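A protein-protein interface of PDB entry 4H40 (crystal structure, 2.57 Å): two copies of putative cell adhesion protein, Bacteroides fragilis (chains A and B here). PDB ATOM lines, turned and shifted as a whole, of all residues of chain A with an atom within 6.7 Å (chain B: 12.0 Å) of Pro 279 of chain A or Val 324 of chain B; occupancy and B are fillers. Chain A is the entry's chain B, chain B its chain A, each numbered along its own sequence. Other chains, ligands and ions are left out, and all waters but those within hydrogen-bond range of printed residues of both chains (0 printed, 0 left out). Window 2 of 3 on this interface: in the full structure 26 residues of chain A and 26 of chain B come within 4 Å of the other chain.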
ATOM      1  N   LEU A 200     -21.506  20.142   1.848  1.00  0.00           N
ATOM      2  CA  LEU A 200     -21.576  19.983   3.288  1.00  0.00           C
ATOM      3  C   LEU A 200     -21.476  18.465   3.590  1.00  0.00           C
ATOM      4  O   LEU A 200     -21.644  17.648   2.667  1.00  0.00           O
ATOM      5  CB  LEU A 200     -22.871  20.588   3.840  1.00  0.00           C
ATOM      6  CG  LEU A 200     -22.991  22.097   3.838  1.00  0.00           C
ATOM      7  CD1 LEU A 200     -24.371  22.510   4.238  1.00  0.00           C
ATOM      8  CD2 LEU A 200     -21.933  22.745   4.716  1.00  0.00           C
ATOM      9  N   ASN A 272     -27.039  20.210  -0.026  1.00  0.00           N
ATOM     10  CA  ASN A 272     -26.490  20.863   1.160  1.00  0.00           C
ATOM     11  C   ASN A 272     -25.116  21.352   0.792  1.00  0.00           C
ATOM     12  O   ASN A 272     -24.189  20.545   0.626  1.00  0.00           O
ATOM     13  CB  ASN A 272     -26.465  19.905   2.333  1.00  0.00           C
ATOM     14  CG  ASN A 272     -27.816  19.333   2.647  1.00  0.00           C
ATOM     15  OD1 ASN A 272     -28.618  19.955   3.317  1.00  0.00           O
ATOM     16  ND2 ASN A 272     -28.096  18.148   2.149  1.00  0.00           N
ATOM     17  N   LEU A 273     -25.006  22.666   0.534  1.00  0.00           N
ATOM     18  CA  LEU A 273     -23.759  23.257   0.059  1.00  0.00           C
ATOM     19  C   LEU A 273     -23.304  24.391   0.945  1.00  0.00           C
ATOM     20  O   LEU A 273     -24.117  25.043   1.611  1.00  0.00           O
ATOM     21  CB  LEU A 273     -23.933  23.783  -1.391  1.00  0.00           C
ATOM     22  CG  LEU A 273     -24.567  22.843  -2.433  1.00  0.00           C
ATOM     23  CD1 LEU A 273     -24.975  23.591  -3.688  1.00  0.00           C
ATOM     24  CD2 LEU A 273     -23.648  21.690  -2.782  1.00  0.00           C
ATOM     25  N   LYS A 274     -21.993  24.639   0.934  1.00  0.00           N
ATOM     26  CA  LYS A 274     -21.363  25.734   1.652  1.00  0.00           C
ATOM     27  C   LYS A 274     -21.024  26.792   0.620  1.00  0.00           C
ATOM     28  O   LYS A 274     -20.030  26.665  -0.080  1.00  0.00           O
ATOM     29  CB  LYS A 274     -20.129  25.242   2.425  1.00  0.00           C
ATOM     30  CG  LYS A 274     -19.664  26.177   3.522  1.00  0.00           C
ATOM     31  CD  LYS A 274     -18.501  25.546   4.244  1.00  0.00           C
ATOM     32  CE  LYS A 274     -18.227  26.218   5.563  1.00  0.00           C
ATOM     33  NZ  LYS A 274     -16.978  25.694   6.174  1.00  0.00           N
ATOM     34  N   VAL A 275     -21.886  27.789   0.476  1.00  0.00           N
ATOM     35  CA  VAL A 275     -21.725  28.889  -0.481  1.00  0.00           C
ATOM     36  C   VAL A 275     -21.101  30.082   0.248  1.00  0.00           C
ATOM     37  O   VAL A 275     -21.639  30.542   1.246  1.00  0.00           O
ATOM     38  CB  VAL A 275     -23.063  29.264  -1.178  1.00  0.00           C
ATOM     39  CG1 VAL A 275     -22.845  30.320  -2.250  1.00  0.00           C
ATOM     40  CG2 VAL A 275     -23.726  28.028  -1.777  1.00  0.00           C
ATOM     41  N   GLY A 277     -18.769  30.323   2.333  1.00  0.00           N
ATOM     42  CA  GLY A 277     -18.566  30.009   3.745  1.00  0.00           C
ATOM     43  C   GLY A 277     -19.811  29.791   4.582  1.00  0.00           C
ATOM     44  O   GLY A 277     -19.696  29.393   5.740  1.00  0.00           O
ATOM     45  N   ASN A 278     -21.006  30.058   4.032  1.00  0.00           N
ATOM     46  CA  ASN A 278     -22.251  29.881   4.781  1.00  0.00           C
ATOM     47  C   ASN A 278     -22.997  28.618   4.327  1.00  0.00           C
ATOM     48  O   ASN A 278     -23.123  28.386   3.117  1.00  0.00           O
ATOM     49  CB  ASN A 278     -23.172  31.100   4.649  1.00  0.00           C
ATOM     50  CG  ASN A 278     -22.480  32.444   4.593  1.00  0.00           C
ATOM     51  OD1 ASN A 278     -22.515  33.134   3.558  1.00  0.00           O
ATOM     52  ND2 ASN A 278     -21.851  32.858   5.700  1.00  0.00           N
ATOM     53  N   PRO A 279     -23.533  27.808   5.276  1.00  0.00           N
ATOM     54  CA  PRO A 279     -24.296  26.610   4.880  1.00  0.00           C
ATOM     55  C   PRO A 279     -25.643  26.973   4.267  1.00  0.00           C
ATOM     56  O   PRO A 279     -26.339  27.864   4.772  1.00  0.00           O
ATOM     57  CB  PRO A 279     -24.486  25.855   6.203  1.00  0.00           C
ATOM     58  CG  PRO A 279     -23.551  26.499   7.176  1.00  0.00           C
ATOM     59  CD  PRO A 279     -23.487  27.929   6.741  1.00  0.00           C
ATOM     60  N   THR A 280     -25.979  26.321   3.139  1.00  0.00           N
ATOM     61  CA  THR A 280     -27.233  26.523   2.405  1.00  0.00           C
ATOM     62  C   THR A 280     -27.868  25.165   2.084  1.00  0.00           C
ATOM     63  O   THR A 280     -27.182  24.151   2.114  1.00  0.00           O
ATOM     64  CB  THR A 280     -27.003  27.319   1.101  1.00  0.00           C
ATOM     65  OG1 THR A 280     -26.248  26.528   0.190  1.00  0.00           O
ATOM     66  CG2 THR A 280     -26.324  28.660   1.312  1.00  0.00           C
ATOM     67  N   GLN A 281     -29.160  25.149   1.760  1.00  0.00           N
ATOM     68  CA  GLN A 281     -29.889  23.958   1.360  1.00  0.00           C
ATOM     69  C   GLN A 281     -30.902  24.357   0.262  1.00  0.00           C
ATOM     70  O   GLN A 281     -31.580  25.370   0.373  1.00  0.00           O
ATOM     71  CB  GLN A 281     -30.559  23.276   2.565  1.00  0.00           C
ATOM     72  CG  GLN A 281     -31.251  21.932   2.254  1.00  0.00           C
ATOM     73  CD  GLN A 281     -31.899  21.296   3.462  1.00  0.00           C
ATOM     74  OE1 GLN A 281     -32.774  21.866   4.121  1.00  0.00           O
ATOM     75  NE2 GLN A 281     -31.508  20.070   3.758  1.00  0.00           N
ATOM     76  N   TYR A 282     -30.957  23.573  -0.805  1.00  0.00           N
ATOM     77  CA  TYR A 282     -31.832  23.780  -1.947  1.00  0.00           C
ATOM     78  C   TYR A 282     -32.546  22.512  -2.262  1.00  0.00           C
ATOM     79  O   TYR A 282     -31.936  21.448  -2.261  1.00  0.00           O
ATOM     80  CB  TYR A 282     -31.041  24.225  -3.197  1.00  0.00           C
ATOM     81  CG  TYR A 282     -30.132  25.393  -2.944  1.00  0.00           C
ATOM     82  CD1 TYR A 282     -30.631  26.687  -2.902  1.00  0.00           C
ATOM     83  CD2 TYR A 282     -28.770  25.208  -2.723  1.00  0.00           C
ATOM     84  CE1 TYR A 282     -29.798  27.773  -2.660  1.00  0.00           C
ATOM     85  CE2 TYR A 282     -27.927  26.288  -2.467  1.00  0.00           C
ATOM     86  CZ  TYR A 282     -28.451  27.569  -2.422  1.00  0.00           C
ATOM     87  OH  TYR A 282     -27.636  28.647  -2.176  1.00  0.00           O
ATOM     88  N   THR B 320     -34.996  27.633  -7.441  1.00  0.00           N
ATOM     89  CA  THR B 320     -35.408  27.430  -6.058  1.00  0.00           C
ATOM     90  C   THR B 320     -34.504  28.341  -5.181  1.00  0.00           C
ATOM     91  O   THR B 320     -33.441  28.773  -5.624  1.00  0.00           O
ATOM     92  CB  THR B 320     -35.409  25.918  -5.728  1.00  0.00           C
ATOM     93  OG1 THR B 320     -36.223  25.656  -4.592  1.00  0.00           O
ATOM     94  CG2 THR B 320     -34.012  25.301  -5.575  1.00  0.00           C
ATOM     95  N   GLU B 321     -34.951  28.674  -3.973  1.00  0.00           N
ATOM     96  CA  GLU B 321     -34.217  29.565  -3.070  1.00  0.00           C
ATOM     97  C   GLU B 321     -33.613  28.805  -1.906  1.00  0.00           C
ATOM     98  O   GLU B 321     -34.013  27.677  -1.623  1.00  0.00           O
ATOM     99  CB  GLU B 321     -35.146  30.675  -2.533  1.00  0.00           C
ATOM    100  CG  GLU B 321     -35.462  31.765  -3.543  1.00  0.00           C
ATOM    101  CD  GLU B 321     -36.246  32.958  -3.028  1.00  0.00           C
ATOM    102  OE1 GLU B 321     -36.052  33.343  -1.851  1.00  0.00           O
ATOM    103  OE2 GLU B 321     -37.016  33.543  -3.824  1.00  0.00           O
ATOM    104  N   ASN B 322     -32.664  29.426  -1.223  1.00  0.00           N
ATOM    105  CA  ASN B 322     -32.050  28.850  -0.045  1.00  0.00           C
ATOM    106  C   ASN B 322     -33.094  28.823   1.053  1.00  0.00           C
ATOM    107  O   ASN B 322     -33.841  29.791   1.227  1.00  0.00           O
ATOM    108  CB  ASN B 322     -30.809  29.651   0.369  1.00  0.00           C
ATOM    109  CG  ASN B 322     -30.125  29.169   1.617  1.00  0.00           C
ATOM    110  OD1 ASN B 322     -30.194  28.001   2.008  1.00  0.00           O
ATOM    111  ND2 ASN B 322     -29.395  30.057   2.242  1.00  0.00           N
ATOM    112  N   VAL B 323     -33.193  27.701   1.735  1.00  0.00           N
ATOM    113  CA  VAL B 323     -34.166  27.505   2.797  1.00  0.00           C
ATOM    114  C   VAL B 323     -33.533  27.908   4.159  1.00  0.00           C
ATOM    115  O   VAL B 323     -34.236  28.450   5.023  1.00  0.00           O
ATOM    116  CB  VAL B 323     -34.757  26.063   2.771  1.00  0.00           C
ATOM    117  CG1 VAL B 323     -35.519  25.815   1.479  1.00  0.00           C
ATOM    118  CG2 VAL B 323     -33.695  24.986   2.955  1.00  0.00           C
ATOM    119  N   VAL B 324     -32.201  27.722   4.299  1.00  0.00           N
ATOM    120  CA  VAL B 324     -31.399  28.062   5.484  1.00  0.00           C
ATOM    121  C   VAL B 324     -31.414  29.594   5.698  1.00  0.00           C
ATOM    122  O   VAL B 324     -32.260  30.119   6.426  1.00  0.00           O
ATOM    123  CB  VAL B 324     -29.951  27.505   5.352  1.00  0.00           C
ATOM    124  CG1 VAL B 324     -29.056  27.995   6.489  1.00  0.00           C
ATOM    125  CG2 VAL B 324     -29.947  25.981   5.289  1.00  0.00           C
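O of Gln 281 of chain A sits at hydrogen-bond distance from N of Val 323 of chain B, 3.1 Å away. N of Gln 281 of chain A is in hydrogen-bond range of OD1 of Asn 322 of chain B.
Hydrophobic or aromatic side chains of chain B that line the printed part of chain A: Val 323 and Val 324. Hydrophobic or aromatic side chains of chain A that line the printed part of chain B: Tyr 282. Among the printed residues, 10 pairs touch across the chains. Among the printed residues, no Asp or Glu carboxylate lies within 4 Å of a Lys or Arg side-chain nitrogen of the other chain.
Among the printed residues, merely in contact across the chains: Pro 279 of chain A with Val 324 of chain B (3.2 Å), Thr 280 of chain A with Asn 322 of chain B (3.3 Å), Tyr 282 of chain A with Asn 322 of chain B (3.6 Å), Gln 281 of chain A with Val 324 of chain B (3.7 Å), Tyr 282 of chain A with Glu 321 of chain B (3.7 Å), Gln 281 of chain A with Glu 321 of chain B (3.9 Å), Thr 280 of chain A with Val 324 of chain B (3.9 Å) and Tyr 282 of chain A with Thr 320 of chain B (3.95 Å).
No position is printed for both chains.
The side-chain hydroxyl (OG1) of Thr 280 of chain A lies close to the side-chain hydroxyl (OH) of Tyr 282 of chain A (3.5 Å). The side-chain amide oxygen (OD1) of Asn 322 of chain B lies within hydrogen-bond range of the backbone NH (N) of Val 324 of chain B, at 3.1 Å. OD1 of Asn 272 of chain A lies within hydrogen-bond range of NE2 of Gln 281 of chain A (2.9 Å). O of Leu 273 of chain A lies within hydrogen-bond range of N of Thr 280 of chain A.
Pro 279 of chain A touches one residue of chain B. Of chain A, only Pro 279, Thr 280 and Gln 281 come within 4 Å of Val 324 of chain B. Val 275 of chain A touches none of the printed residues of chain B. No residue of chain B comes within 4 Å of Gly 277 of chain A. Asn 278 of chain A touches none of the printed residues of chain B. Of chain B, only Asn 322 (3.3 Å) and Val 324 (3.9 Å) come within 4 Å of Thr 280 of chain A. Gln 281 of chain A touches just these residues of chain B: Glu 321 (3.9 Å), Asn 322 (3.0 Å), Val 323 (3.1 Å) and Val 324 (3.7 Å). Printed residues of chain A within 4 Å of Thr 320 of chain B: Tyr 282 (3.95 Å). Printed residues of chain B within 4 Å of Tyr 282 of chain A: Thr 320, Glu 321 and Asn 322. Of the printed residues of chain A, Asn 322 of chain B touches Thr 280, Gln 281 and Tyr 282. Printed residues of chain A within 4 Å of Glu 321 of chain B: Gln 281 and Tyr 282. Printed residues of chain A within 4 Å of Val 323 of chain B: Gln 281 (3.1 Å). The nearest residue of chain B that does not touch Pro 279 of chain A is Asn 322 of chain B (4.5 Å).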
